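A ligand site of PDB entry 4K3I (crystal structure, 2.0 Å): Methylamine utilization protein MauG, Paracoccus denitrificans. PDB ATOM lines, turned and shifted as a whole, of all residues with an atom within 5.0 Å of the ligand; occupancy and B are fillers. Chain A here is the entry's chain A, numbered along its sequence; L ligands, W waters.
Water W5 lies within hydrogen-bond range of the backbone carbonyl oxygen (O) of Thr 69 and an oxygen (O1) of the ligand. Water W3 bridges O1 of the ligand (2.9 Å) and NE2 of Gln 91 (3.1 Å). Water W1 lies within hydrogen-bond range of O of Arg 65 (2.7 Å) and N of Ser 54 (2.8 Å). Water W6 lies within hydrogen-bond range of the backbone carbonyl oxygen (O) of Ser 54, the backbone carbonyl oxygen (O) of Val 112 and the backbone NH (N) of Gly 56.
SG of Cys 31 is covalently linked to C18 of the ligand (1.8 Å). SG of Cys 34 is covalently linked to C25 of the ligand. An iron atom (FE1) of the ligand is bound by a ring nitrogen (NE2) of His 35, 2.1 Å away. The backbone NH of Phe 92 sits at hydrogen-bond distance from an oxygen (O2) of the ligand, 2.7 Å away. The guanidinium group (NH2) of Arg 96 lies within salt-bridge range of an oxygen (O3) of the ligand, 2.8 Å away. N of Trp 93 sits at hydrogen-bond distance from O4 of the ligand. An oxygen (O3) of the ligand is in salt-bridge range of the guanidinium group (NH1) of Arg 65 (3.1 Å). The side-chain amino group (NZ) of Lys 265 is in salt-bridge range of an oxygen (O2) of the ligand (3.1 Å).
NE2 of Gln 103 lies close to N1 of the ligand (3.2 Å). Gln 29 touches the ligand. O of Ser 30 touches C24 of the ligand, at 3.6 Å. Ser 54 touches the ligand (CB to C25, 3.8 Å). Val 55 touches the ligand (O to C26, 3.6 Å). Asn 66 touches the ligand. OG1 of Thr 67 touches C4 of the ligand, 3.3 Å away. Pro 68 touches the ligand. CD2 of Leu 70 touches C7 of the ligand, 3.5 Å away. Gln 91 touches the ligand (NE2 to C11, 3.5 Å). CD2 of Leu 100 touches C9 of the ligand, at 3.4 Å. Ala 104 touches the ligand. Pro 107 touches the ligand (CG to C16, 3.4 Å). Glu 113 touches the ligand. CG of Met 114 touches C24 of the ligand, 3.7 Å away. CD1 of Leu 159 touches C19 of the ligand (3.99 Å). Gln 163 touches the ligand. Hydrophobic or aromatic side chains within 4 Å of the ligand: His 35, Pro 68, Leu 70, Phe 92, Trp 93, Leu 100, Pro 107, Met 114 and Leu 159. Within 4 Å of the ligand: Gln 29, Ser 30, Cys 31, Cys 34, His 35, Ser 54, Val 55, Arg 65, Asn 66, Thr 67, Pro 68, Leu 70, Gln 91, Phe 92, Trp 93, Arg 96, Leu 100, Gln 103, Ala 104, Pro 107, Glu 113, Met 114, Leu 159, Gln 163 and Lys 265. The nearest printed residue that does not touch the ligand is Gly 56 (4.001 Å).
O of Phe 18 sits at hydrogen-bond distance from N of Cys 31 (3.2 Å). ND1 of His 35 is in hydrogen-bond range of O of Pro 68 (3.0 Å). The guanidinium group (NH2) of Arg 96 lies within salt-bridge range of the side-chain carboxylate (OD1) of Asp 94, at 3.0 Å. O of Trp 93 is in hydrogen-bond range of N of Lys 265 (2.8 Å). The indole nitrogen (NE1) of Trp 93 is in hydrogen-bond range of the backbone carbonyl oxygen (O) of Asn 66. OE1 of Gln 91 sits close to O of Ala 73 (3.1 Å). The backbone carbonyl oxygen (O) of Glu 113 sits at hydrogen-bond distance from the side-chain amide nitrogen (NE2) of Gln 29, 3.1 Å away. N of Met 114 lies close to NE2 of Gln 29, at 3.4 Å.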
ATOM      1  N   PHE A  18     -20.460  22.393 -15.727  1.00  0.00           N
ATOM      2  CA  PHE A  18     -20.291  22.722 -17.128  1.00  0.00           C
ATOM      3  C   PHE A  18     -18.875  22.988 -17.518  1.00  0.00           C
ATOM      4  O   PHE A  18     -18.471  22.659 -18.645  1.00  0.00           O
ATOM      5  CB  PHE A  18     -21.169  23.941 -17.502  1.00  0.00           C
ATOM      6  CG  PHE A  18     -21.311  24.175 -19.008  1.00  0.00           C
ATOM      7  CD1 PHE A  18     -22.194  23.386 -19.775  1.00  0.00           C
ATOM      8  CD2 PHE A  18     -20.570  25.194 -19.638  1.00  0.00           C
ATOM      9  CE1 PHE A  18     -22.333  23.616 -21.138  1.00  0.00           C
ATOM     10  CE2 PHE A  18     -20.668  25.399 -21.018  1.00  0.00           C
ATOM     11  CZ  PHE A  18     -21.564  24.593 -21.780  1.00  0.00           C
ATOM     12  N   GLN A  29     -11.028  17.660 -20.487  1.00  0.00           N
ATOM     13  CA  GLN A  29     -12.106  18.348 -21.128  1.00  0.00           C
ATOM     14  C   GLN A  29     -13.393  18.444 -20.318  1.00  0.00           C
ATOM     15  O   GLN A  29     -13.703  17.577 -19.462  1.00  0.00           O
ATOM     16  CB  GLN A  29     -12.261  17.791 -22.557  1.00  0.00           C
ATOM     17  CG  GLN A  29     -13.439  16.984 -22.872  1.00  0.00           C
ATOM     18  CD  GLN A  29     -13.428  16.406 -24.288  1.00  0.00           C
ATOM     19  OE1 GLN A  29     -12.817  16.909 -25.242  1.00  0.00           O
ATOM     20  NE2 GLN A  29     -14.115  15.312 -24.411  1.00  0.00           N
ATOM     21  N   SER A  30     -14.083  19.580 -20.511  1.00  0.00           N
ATOM     22  CA  SER A  30     -15.375  19.840 -19.902  1.00  0.00           C
ATOM     23  C   SER A  30     -16.417  20.045 -21.018  1.00  0.00           C
ATOM     24  O   SER A  30     -16.032  20.106 -22.194  1.00  0.00           O
ATOM     25  CB  SER A  30     -15.259  21.102 -19.050  1.00  0.00           C
ATOM     26  OG  SER A  30     -15.140  22.271 -19.852  1.00  0.00           O
ATOM     27  N   CYS A  31     -17.679  20.227 -20.649  1.00  0.00           N
ATOM     28  CA  CYS A  31     -18.715  20.596 -21.633  1.00  0.00           C
ATOM     29  C   CYS A  31     -18.266  21.818 -22.409  1.00  0.00           C
ATOM     30  O   CYS A  31     -18.409  21.906 -23.649  1.00  0.00           O
ATOM     31  CB  CYS A  31     -20.045  20.928 -20.975  1.00  0.00           C
ATOM     32  SG  CYS A  31     -20.670  19.660 -19.832  1.00  0.00           S
ATOM     33  N   CYS A  34     -15.859  21.775 -25.803  1.00  0.00           N
ATOM     34  CA  CYS A  34     -16.524  21.663 -27.092  1.00  0.00           C
ATOM     35  C   CYS A  34     -17.631  22.694 -27.325  1.00  0.00           C
ATOM     36  O   CYS A  34     -17.831  23.176 -28.452  1.00  0.00           O
ATOM     37  CB  CYS A  34     -17.127  20.275 -27.208  1.00  0.00           C
ATOM     38  SG  CYS A  34     -15.923  18.960 -27.331  1.00  0.00           S
ATOM     39  N   HIS A  35     -18.357  23.021 -26.268  1.00  0.00           N
ATOM     40  CA  HIS A  35     -19.384  24.037 -26.307  1.00  0.00           C
ATOM     41  C   HIS A  35     -18.810  25.366 -25.671  1.00  0.00           C
ATOM     42  O   HIS A  35     -19.106  25.809 -24.515  1.00  0.00           O
ATOM     43  CB  HIS A  35     -20.638  23.538 -25.613  1.00  0.00           C
ATOM     44  CG  HIS A  35     -21.231  22.284 -26.223  1.00  0.00           C
ATOM     45  ND1 HIS A  35     -21.942  22.279 -27.401  1.00  0.00           N
ATOM     46  CD2 HIS A  35     -21.242  21.019 -25.779  1.00  0.00           C
ATOM     47  CE1 HIS A  35     -22.371  21.044 -27.645  1.00  0.00           C
ATOM     48  NE2 HIS A  35     -21.983  20.262 -26.660  1.00  0.00           N
ATOM     49  N   ARG A  45     -11.735  24.419 -31.850  1.00  0.00           N
ATOM     50  CA  ARG A  45     -10.503  23.642 -32.026  1.00  0.00           C
ATOM     51  C   ARG A  45     -10.415  22.951 -33.404  1.00  0.00           C
ATOM     52  O   ARG A  45     -11.357  22.375 -33.919  1.00  0.00           O
ATOM     53  CB  ARG A  45     -10.373  22.555 -30.917  1.00  0.00           C
ATOM     54  CG  ARG A  45     -10.383  23.174 -29.538  1.00  0.00           C
ATOM     55  CD  ARG A  45     -10.424  22.152 -28.421  1.00  0.00           C
ATOM     56  NE  ARG A  45     -11.582  21.304 -28.580  1.00  0.00           N
ATOM     57  CZ  ARG A  45     -11.642  20.012 -28.309  1.00  0.00           C
ATOM     58  NH1 ARG A  45     -10.604  19.399 -27.761  1.00  0.00           N
ATOM     59  NH2 ARG A  45     -12.775  19.311 -28.536  1.00  0.00           N
ATOM     60  N   SER A  54     -15.427  17.231 -33.547  1.00  0.00           N
ATOM     61  CA  SER A  54     -14.665  17.561 -32.368  1.00  0.00           C
ATOM     62  C   SER A  54     -13.887  16.353 -31.876  1.00  0.00           C
ATOM     63  O   SER A  54     -14.260  15.160 -32.063  1.00  0.00           O
ATOM     64  CB  SER A  54     -15.578  18.057 -31.241  1.00  0.00           C
ATOM     65  OG  SER A  54     -16.206  19.286 -31.554  1.00  0.00           O
ATOM     66  N   VAL A  55     -12.834  16.671 -31.184  1.00  0.00           N
ATOM     67  CA  VAL A  55     -11.914  15.648 -30.668  1.00  0.00           C
ATOM     68  C   VAL A  55     -12.183  15.422 -29.195  1.00  0.00           C
ATOM     69  O   VAL A  55     -12.283  16.382 -28.412  1.00  0.00           O
ATOM     70  CB  VAL A  55     -10.454  16.115 -30.837  1.00  0.00           C
ATOM     71  CG1 VAL A  55      -9.515  15.046 -30.289  1.00  0.00           C
ATOM     72  CG2 VAL A  55     -10.135  16.404 -32.298  1.00  0.00           C
ATOM     73  N   GLY A  56     -12.339  14.159 -28.776  1.00  0.00           N
ATOM     74  CA  GLY A  56     -12.566  13.880 -27.377  1.00  0.00           C
ATOM     75  C   GLY A  56     -11.350  13.951 -26.433  1.00  0.00           C
ATOM     76  O   GLY A  56     -10.207  14.323 -26.828  1.00  0.00           O
ATOM     77  N   ARG A  65     -20.439  13.900 -36.195  1.00  0.00           N
ATOM     78  CA  ARG A  65     -21.316  15.044 -36.338  1.00  0.00           C
ATOM     79  C   ARG A  65     -20.656  16.299 -35.769  1.00  0.00           C
ATOM     80  O   ARG A  65     -19.794  16.246 -34.882  1.00  0.00           O
ATOM     81  CB  ARG A  65     -22.659  14.778 -35.635  1.00  0.00           C
ATOM     82  CG  ARG A  65     -23.395  13.588 -36.185  1.00  0.00           C
ATOM     83  CD  ARG A  65     -24.774  13.462 -35.646  1.00  0.00           C
ATOM     84  NE  ARG A  65     -25.556  12.358 -36.262  1.00  0.00           N
ATOM     85  CZ  ARG A  65     -26.508  11.708 -35.621  1.00  0.00           C
ATOM     86  NH1 ARG A  65     -26.808  12.054 -34.388  1.00  0.00           N
ATOM     87  NH2 ARG A  65     -27.179  10.711 -36.190  1.00  0.00           N
ATOM     88  N   ASN A  66     -21.056  17.458 -36.321  1.00  0.00           N
ATOM     89  CA  ASN A  66     -20.625  18.777 -35.871  1.00  0.00           C
ATOM     90  C   ASN A  66     -21.223  19.093 -34.514  1.00  0.00           C
ATOM     91  O   ASN A  66     -22.440  18.872 -34.240  1.00  0.00           O
ATOM     92  CB  ASN A  66     -21.067  19.792 -36.918  1.00  0.00           C
ATOM     93  CG  ASN A  66     -20.658  21.234 -36.631  1.00  0.00           C
ATOM     94  OD1 ASN A  66     -21.508  22.081 -36.471  1.00  0.00           O
ATOM     95  ND2 ASN A  66     -19.362  21.514 -36.654  1.00  0.00           N
ATOM     96  N   THR A  67     -20.409  19.650 -33.647  1.00  0.00           N
ATOM     97  CA  THR A  67     -20.876  20.085 -32.306  1.00  0.00           C
ATOM     98  C   THR A  67     -21.805  21.290 -32.458  1.00  0.00           C
ATOM     99  O   THR A  67     -21.361  22.377 -32.941  1.00  0.00           O
ATOM    100  CB  THR A  67     -19.647  20.446 -31.451  1.00  0.00           C
ATOM    101  OG1 THR A  67     -18.857  19.264 -31.270  1.00  0.00           O
ATOM    102  CG2 THR A  67     -20.040  21.104 -30.060  1.00  0.00           C
ATOM    103  N   PRO A  68     -23.089  21.127 -32.082  1.00  0.00           N
ATOM    104  CA  PRO A  68     -24.036  22.208 -32.167  1.00  0.00           C
ATOM    105  C   PRO A  68     -23.943  23.123 -31.018  1.00  0.00           C
ATOM    106  O   PRO A  68     -23.448  22.736 -29.918  1.00  0.00           O
ATOM    107  CB  PRO A  68     -25.393  21.512 -32.118  1.00  0.00           C
ATOM    108  CG  PRO A  68     -25.138  20.351 -31.160  1.00  0.00           C
ATOM    109  CD  PRO A  68     -23.714  19.922 -31.464  1.00  0.00           C
ATOM    110  N   THR A  69     -24.413  24.340 -31.267  1.00  0.00           N
ATOM    111  CA  THR A  69     -24.628  25.300 -30.191  1.00  0.00           C
ATOM    112  C   THR A  69     -25.576  24.815 -29.130  1.00  0.00           C
ATOM    113  O   THR A  69     -26.593  24.092 -29.404  1.00  0.00           O
ATOM    114  CB  THR A  69     -25.115  26.675 -30.731  1.00  0.00           C
ATOM    115  OG1 THR A  69     -25.116  27.646 -29.711  1.00  0.00           O
ATOM    116  CG2 THR A  69     -26.555  26.571 -31.229  1.00  0.00           C
ATOM    117  N   LEU A  70     -25.313  25.207 -27.892  1.00  0.00           N
ATOM    118  CA  LEU A  70     -26.289  25.033 -26.793  1.00  0.00           C
ATOM    119  C   LEU A  70     -27.162  26.258 -26.587  1.00  0.00           C
ATOM    120  O   LEU A  70     -28.068  26.222 -25.777  1.00  0.00           O
ATOM    121  CB  LEU A  70     -25.592  24.746 -25.472  1.00  0.00           C
ATOM    122  CG  LEU A  70     -24.598  23.593 -25.604  1.00  0.00           C
ATOM    123  CD1 LEU A  70     -23.983  23.356 -24.249  1.00  0.00           C
ATOM    124  CD2 LEU A  70     -25.325  22.383 -26.132  1.00  0.00           C
ATOM    125  N   ALA A  73     -31.140  25.979 -26.954  1.00  0.00           N
ATOM    126  CA  ALA A  73     -31.516  24.516 -26.911  1.00  0.00           C
ATOM    127  C   ALA A  73     -32.600  24.259 -25.893  1.00  0.00           C
ATOM    128  O   ALA A  73     -33.353  23.256 -26.021  1.00  0.00           O
ATOM    129  CB  ALA A  73     -30.288  23.646 -26.597  1.00  0.00           C
ATOM    130  N   GLN A  91     -33.299  16.109 -28.421  1.00  0.00           N
ATOM    131  CA  GLN A  91     -31.963  16.614 -28.378  1.00  0.00           C
ATOM    132  C   GLN A  91     -31.028  15.642 -29.151  1.00  0.00           C
ATOM    133  O   GLN A  91     -31.291  14.426 -29.263  1.00  0.00           O
ATOM    134  CB  GLN A  91     -31.520  16.868 -26.905  1.00  0.00           C
ATOM    135  CG  GLN A  91     -32.263  17.986 -26.110  1.00  0.00           C
ATOM    136  CD  GLN A  91     -32.142  19.372 -26.689  1.00  0.00           C
ATOM    137  OE1 GLN A  91     -33.011  20.204 -26.512  1.00  0.00           O
ATOM    138  NE2 GLN A  91     -31.053  19.648 -27.310  1.00  0.00           N
ATOM    139  N   PHE A  92     -29.958  16.240 -29.708  1.00  0.00           N
ATOM    140  CA  PHE A  92     -28.991  15.694 -30.631  1.00  0.00           C
ATOM    141  C   PHE A  92     -29.602  15.878 -32.023  1.00  0.00           C
ATOM    142  O   PHE A  92     -30.822  16.005 -32.197  1.00  0.00           O
ATOM    143  CB  PHE A  92     -28.639  14.175 -30.408  1.00  0.00           C
ATOM    144  CG  PHE A  92     -27.824  13.864 -29.180  1.00  0.00           C
ATOM    145  CD1 PHE A  92     -26.527  14.367 -29.044  1.00  0.00           C
ATOM    146  CD2 PHE A  92     -28.300  12.950 -28.224  1.00  0.00           C
ATOM    147  CE1 PHE A  92     -25.752  14.015 -27.974  1.00  0.00           C
ATOM    148  CE2 PHE A  92     -27.490  12.591 -27.162  1.00  0.00           C
ATOM    149  CZ  PHE A  92     -26.217  13.113 -27.047  1.00  0.00           C
ATOM    150  N   TRP A  93     -28.748  15.869 -33.036  1.00  0.00           N
ATOM    151  CA  TRP A  93     -29.164  16.130 -34.394  1.00  0.00           C
ATOM    152  C   TRP A  93     -30.178  15.055 -34.867  1.00  0.00           C
ATOM    153  O   TRP A  93     -30.910  15.306 -35.823  1.00  0.00           O
ATOM    154  CB  TRP A  93     -27.972  16.073 -35.329  1.00  0.00           C
ATOM    155  CG  TRP A  93     -27.018  17.203 -35.290  1.00  0.00           C
ATOM    156  CD1 TRP A  93     -25.790  17.227 -34.669  1.00  0.00           C
ATOM    157  CD2 TRP A  93     -27.101  18.370 -36.056  1.00  0.00           C
ATOM    158  NE1 TRP A  93     -25.139  18.416 -34.952  1.00  0.00           N
ATOM    159  CE2 TRP A  93     -25.929  19.143 -35.801  1.00  0.00           C
ATOM    160  CE3 TRP A  93     -28.051  18.863 -36.960  1.00  0.00           C
ATOM    161  CZ2 TRP A  93     -25.689  20.392 -36.415  1.00  0.00           C
ATOM    162  CZ3 TRP A  93     -27.830  20.097 -37.556  1.00  0.00           C
ATOM    163  CH2 TRP A  93     -26.642  20.844 -37.282  1.00  0.00           C
ATOM    164  N   ASP A  94     -30.180  13.881 -34.215  1.00  0.00           N
ATOM    165  CA  ASP A  94     -31.128  12.809 -34.550  1.00  0.00           C
ATOM    166  C   ASP A  94     -32.180  12.625 -33.491  1.00  0.00           C
ATOM    167  O   ASP A  94     -32.899  11.687 -33.559  1.00  0.00           O
ATOM    168  CB  ASP A  94     -30.429  11.496 -34.786  1.00  0.00           C
ATOM    169  CG  ASP A  94     -29.620  11.043 -33.568  1.00  0.00           C
ATOM    170  OD1 ASP A  94     -29.801  11.584 -32.447  1.00  0.00           O
ATOM    171  OD2 ASP A  94     -28.826  10.111 -33.793  1.00  0.00           O
ATOM    172  N   ARG A  96     -32.293  11.549 -30.545  1.00  0.00           N
ATOM    173  CA  ARG A  96     -32.276  10.280 -29.807  1.00  0.00           C
ATOM    174  C   ARG A  96     -32.389  10.479 -28.289  1.00  0.00           C
ATOM    175  O   ARG A  96     -32.616   9.536 -27.578  1.00  0.00           O
ATOM    176  CB  ARG A  96     -31.079   9.404 -30.169  1.00  0.00           C
ATOM    177  CG  ARG A  96     -29.753   9.877 -29.618  1.00  0.00           C
ATOM    178  CD  ARG A  96     -28.621   9.037 -30.154  1.00  0.00           C
ATOM    179  NE  ARG A  96     -27.325   9.478 -29.681  1.00  0.00           N
ATOM    180  CZ  ARG A  96     -26.636  10.490 -30.207  1.00  0.00           C
ATOM    181  NH1 ARG A  96     -25.458  10.739 -29.731  1.00  0.00           N
ATOM    182  NH2 ARG A  96     -27.085  11.215 -31.233  1.00  0.00           N
ATOM    183  N   LEU A 100     -33.029  17.753 -22.488  1.00  0.00           N
ATOM    184  CA  LEU A 100     -31.698  18.068 -22.033  1.00  0.00           C
ATOM    185  C   LEU A 100     -31.246  17.134 -20.893  1.00  0.00           C
ATOM    186  O   LEU A 100     -30.093  16.767 -20.835  1.00  0.00           O
ATOM    187  CB  LEU A 100     -31.614  19.515 -21.546  1.00  0.00           C
ATOM    188  CG  LEU A 100     -31.800  20.614 -22.642  1.00  0.00           C
ATOM    189  CD1 LEU A 100     -32.015  22.018 -22.037  1.00  0.00           C
ATOM    190  CD2 LEU A 100     -30.631  20.587 -23.593  1.00  0.00           C
ATOM    191  N   GLN A 103     -30.082  14.020 -22.263  1.00  0.00           N
ATOM    192  CA  GLN A 103     -28.864  14.198 -23.069  1.00  0.00           C
ATOM    193  C   GLN A 103     -27.591  14.333 -22.235  1.00  0.00           C
ATOM    194  O   GLN A 103     -26.511  13.866 -22.614  1.00  0.00           O
ATOM    195  CB  GLN A 103     -28.974  15.412 -23.933  1.00  0.00           C
ATOM    196  CG  GLN A 103     -27.835  15.540 -24.929  1.00  0.00           C
ATOM    197  CD  GLN A 103     -26.592  16.124 -24.338  1.00  0.00           C
ATOM    198  OE1 GLN A 103     -26.627  16.835 -23.345  1.00  0.00           O
ATOM    199  NE2 GLN A 103     -25.495  15.937 -25.021  1.00  0.00           N
ATOM    200  N   ALA A 104     -27.696  15.031 -21.107  1.00  0.00           N
ATOM    201  CA  ALA A 104     -26.484  15.529 -20.429  1.00  0.00           C
ATOM    202  C   ALA A 104     -25.486  14.474 -19.983  1.00  0.00           C
ATOM    203  O   ALA A 104     -24.274  14.706 -19.996  1.00  0.00           O
ATOM    204  CB  ALA A 104     -26.881  16.438 -19.277  1.00  0.00           C
ATOM    205  N   PRO A 107     -22.502  12.674 -23.149  1.00  0.00           N
ATOM    206  CA  PRO A 107     -21.064  12.988 -23.475  1.00  0.00           C
ATOM    207  C   PRO A 107     -20.085  12.477 -22.384  1.00  0.00           C
ATOM    208  O   PRO A 107     -18.908  12.144 -22.656  1.00  0.00           O
ATOM    209  CB  PRO A 107     -21.037  14.529 -23.559  1.00  0.00           C
ATOM    210  CG  PRO A 107     -22.450  14.987 -23.520  1.00  0.00           C
ATOM    211  CD  PRO A 107     -23.378  13.854 -23.219  1.00  0.00           C
ATOM    212  N   MET A 108     -20.584  12.373 -21.157  1.00  0.00           N
ATOM    213  CA  MET A 108     -19.715  12.001 -20.020  1.00  0.00           C
ATOM    214  C   MET A 108     -19.220  10.587 -20.188  1.00  0.00           C
ATOM    215  O   MET A 108     -18.042  10.276 -19.917  1.00  0.00           O
ATOM    216  CB  MET A 108     -20.407  12.172 -18.696  1.00  0.00           C
ATOM    217  CG  MET A 108     -20.787  13.564 -18.286  1.00  0.00           C
ATOM    218  SD  MET A 108     -21.732  13.408 -16.739  1.00  0.00           S
ATOM    219  CE  MET A 108     -22.598  14.934 -16.682  1.00  0.00           C
ATOM    220  N   VAL A 112     -15.823   8.369 -27.291  1.00  0.00           N
ATOM    221  CA  VAL A 112     -15.321   9.360 -28.247  1.00  0.00           C
ATOM    222  C   VAL A 112     -15.357  10.799 -27.749  1.00  0.00           C
ATOM    223  O   VAL A 112     -14.751  11.650 -28.340  1.00  0.00           O
ATOM    224  CB  VAL A 112     -15.819   9.192 -29.696  1.00  0.00           C
ATOM    225  CG1 VAL A 112     -16.355   7.814 -30.026  1.00  0.00           C
ATOM    226  CG2 VAL A 112     -16.624  10.329 -30.251  1.00  0.00           C
ATOM    227  N   GLU A 113     -16.034  11.042 -26.649  1.00  0.00           N
ATOM    228  CA  GLU A 113     -16.052  12.358 -26.021  1.00  0.00           C
ATOM    229  C   GLU A 113     -15.278  12.386 -24.662  1.00  0.00           C
ATOM    230  O   GLU A 113     -14.040  12.270 -24.630  1.00  0.00           O
ATOM    231  CB  GLU A 113     -17.510  12.866 -25.986  1.00  0.00           C
ATOM    232  CG  GLU A 113     -18.055  13.020 -27.422  1.00  0.00           C
ATOM    233  CD  GLU A 113     -19.559  13.258 -27.575  1.00  0.00           C
ATOM    234  OE1 GLU A 113     -20.343  12.746 -26.758  1.00  0.00           O
ATOM    235  OE2 GLU A 113     -19.970  13.896 -28.602  1.00  0.00           O
ATOM    236  N   MET A 114     -16.005  12.566 -23.574  1.00  0.00           N
ATOM    237  CA  MET A 114     -15.426  12.727 -22.284  1.00  0.00           C
ATOM    238  C   MET A 114     -14.913  11.402 -21.702  1.00  0.00           C
ATOM    239  O   MET A 114     -14.045  11.419 -20.816  1.00  0.00           O
ATOM    240  CB  MET A 114     -16.380  13.423 -21.349  1.00  0.00           C
ATOM    241  CG  MET A 114     -16.806  14.771 -21.920  1.00  0.00           C
ATOM    242  SD  MET A 114     -17.979  15.695 -20.938  1.00  0.00           S
ATOM    243  CE  MET A 114     -16.975  16.182 -19.562  1.00  0.00           C
ATOM    244  N   LEU A 159     -27.023  20.163 -14.997  1.00  0.00           N
ATOM    245  CA  LEU A 159     -26.615  20.634 -16.284  1.00  0.00           C
ATOM    246  C   LEU A 159     -27.753  21.139 -17.148  1.00  0.00           C
ATOM    247  O   LEU A 159     -27.601  22.179 -17.759  1.00  0.00           O
ATOM    248  CB  LEU A 159     -25.746  19.618 -17.025  1.00  0.00           C
ATOM    249  CG  LEU A 159     -24.310  19.552 -16.462  1.00  0.00           C
ATOM    250  CD1 LEU A 159     -23.784  18.169 -16.786  1.00  0.00           C
ATOM    251  CD2 LEU A 159     -23.360  20.600 -17.005  1.00  0.00           C
ATOM    252  N   GLN A 163     -28.506  25.073 -18.481  1.00  0.00           N
ATOM    253  CA  GLN A 163     -28.735  25.414 -19.925  1.00  0.00           C
ATOM    254  C   GLN A 163     -30.074  26.157 -20.174  1.00  0.00           C
ATOM    255  O   GLN A 163     -30.270  26.754 -21.248  1.00  0.00           O
ATOM    256  CB  GLN A 163     -28.671  24.146 -20.814  1.00  0.00           C
ATOM    257  CG  GLN A 163     -27.250  23.582 -20.926  1.00  0.00           C
ATOM    258  CD  GLN A 163     -27.260  22.191 -21.508  1.00  0.00           C
ATOM    259  OE1 GLN A 163     -27.354  21.140 -20.776  1.00  0.00           O
ATOM    260  NE2 GLN A 163     -27.275  22.147 -22.826  1.00  0.00           N
ATOM    261  N   LYS A 265     -32.827  16.907 -37.153  1.00  0.00           N
ATOM    262  CA  LYS A 265     -33.503  18.017 -36.514  1.00  0.00           C
ATOM    263  C   LYS A 265     -33.171  19.346 -37.125  1.00  0.00           C
ATOM    264  O   LYS A 265     -31.997  19.680 -37.319  1.00  0.00           O
ATOM    265  CB  LYS A 265     -33.184  18.025 -35.040  1.00  0.00           C
ATOM    266  CG  LYS A 265     -33.805  19.193 -34.293  1.00  0.00           C
ATOM    267  CD  LYS A 265     -33.975  18.932 -32.771  1.00  0.00           C
ATOM    268  CE  LYS A 265     -32.684  18.696 -32.080  1.00  0.00           C
ATOM    269  NZ  LYS A 265     -31.708  19.742 -32.283  1.00  0.00           N
HETATM  270 FE1  LIG L   1     -22.309  18.230 -26.401  1.00  0.00          FE
HETATM  271  C1  LIG L   1     -24.678  17.789 -28.760  1.00  0.00           C
HETATM  272  C2  LIG L   1     -24.696  19.228 -24.130  1.00  0.00           C
HETATM  273  C3  LIG L   1     -20.062  17.773 -23.879  1.00  0.00           C
HETATM  274  C4  LIG L   1     -19.797  17.417 -28.679  1.00  0.00           C
HETATM  275  N1  LIG L   1     -24.310  18.593 -26.465  1.00  0.00           N
HETATM  276  C5  LIG L   1     -25.130  18.286 -27.470  1.00  0.00           C
HETATM  277  C6  LIG L   1     -26.538  18.666 -27.213  1.00  0.00           C
HETATM  278  C7  LIG L   1     -26.536  19.075 -25.889  1.00  0.00           C
HETATM  279  C8  LIG L   1     -25.143  18.888 -25.465  1.00  0.00           C
HETATM  280  C9  LIG L   1     -27.704  19.583 -25.102  1.00  0.00           C
HETATM  281  C10 LIG L   1     -27.741  18.598 -28.113  1.00  0.00           C
HETATM  282  C11 LIG L   1     -27.947  19.898 -28.868  1.00  0.00           C
HETATM  283  C12 LIG L   1     -28.871  19.831 -30.115  1.00  0.00           C
HETATM  284  O1  LIG L   1     -29.172  20.849 -30.756  1.00  0.00           O
HETATM  285  O2  LIG L   1     -29.314  18.756 -30.516  1.00  0.00           O
HETATM  286  N2  LIG L   1     -22.343  18.575 -24.380  1.00  0.00           N
HETATM  287  C13 LIG L   1     -23.402  18.844 -23.608  1.00  0.00           C
HETATM  288  C14 LIG L   1     -23.091  18.864 -22.194  1.00  0.00           C
HETATM  289  C15 LIG L   1     -21.777  18.432 -22.109  1.00  0.00           C
HETATM  290  C16 LIG L   1     -21.420  18.199 -23.507  1.00  0.00           C
HETATM  291  C17 LIG L   1     -24.133  19.273 -21.204  1.00  0.00           C
HETATM  292  C18 LIG L   1     -20.949  18.198 -20.879  1.00  0.00           C
HETATM  293  C19 LIG L   1     -21.607  17.184 -19.980  1.00  0.00           C
HETATM  294  N3  LIG L   1     -20.274  17.744 -26.310  1.00  0.00           N
HETATM  295  C20 LIG L   1     -19.542  17.570 -25.219  1.00  0.00           C
HETATM  296  C21 LIG L   1     -18.098  17.519 -25.482  1.00  0.00           C
HETATM  297  C22 LIG L   1     -17.977  17.434 -26.860  1.00  0.00           C
HETATM  298  C23 LIG L   1     -19.399  17.475 -27.303  1.00  0.00           C
HETATM  299  C24 LIG L   1     -17.019  17.509 -24.436  1.00  0.00           C
HETATM  300  C25 LIG L   1     -16.740  17.349 -27.724  1.00  0.00           C
HETATM  301  C26 LIG L   1     -15.812  16.215 -27.506  1.00  0.00           C
HETATM  302  N4  LIG L   1     -22.285  17.799 -28.405  1.00  0.00           N
HETATM  303  C27 LIG L   1     -21.244  17.360 -29.110  1.00  0.00           C
HETATM  304  C28 LIG L   1     -21.646  16.861 -30.392  1.00  0.00           C
HETATM  305  C29 LIG L   1     -23.031  16.909 -30.415  1.00  0.00           C
HETATM  306  C30 LIG L   1     -23.339  17.470 -29.158  1.00  0.00           C
HETATM  307  C31 LIG L   1     -20.694  16.369 -31.432  1.00  0.00           C
HETATM  308  C32 LIG L   1     -23.862  16.465 -31.527  1.00  0.00           C
HETATM  309  C33 LIG L   1     -23.810  14.965 -31.423  1.00  0.00           C
HETATM  310  C34 LIG L   1     -24.993  14.227 -32.072  1.00  0.00           C
HETATM  311  O3  LIG L   1     -24.986  12.976 -32.013  1.00  0.00           O
HETATM  312  O4  LIG L   1     -25.951  14.826 -32.614  1.00  0.00           O
HETATM  313  O   HOH W   1     -17.764  15.769 -33.108  1.00  0.00           O
HETATM  314  O   HOH W   2     -24.284   9.717 -32.913  1.00  0.00           O
HETATM  315  O   HOH W   3     -31.409  21.978 -29.354  1.00  0.00           O
HETATM  316  O   HOH W   4     -28.132  19.423 -33.222  1.00  0.00           O
HETATM  317  O   HOH W   5     -28.708  23.405 -30.744  1.00  0.00           O
HETATM  318  O   HOH W   6     -15.533  13.818 -29.983  1.00  0.00           O
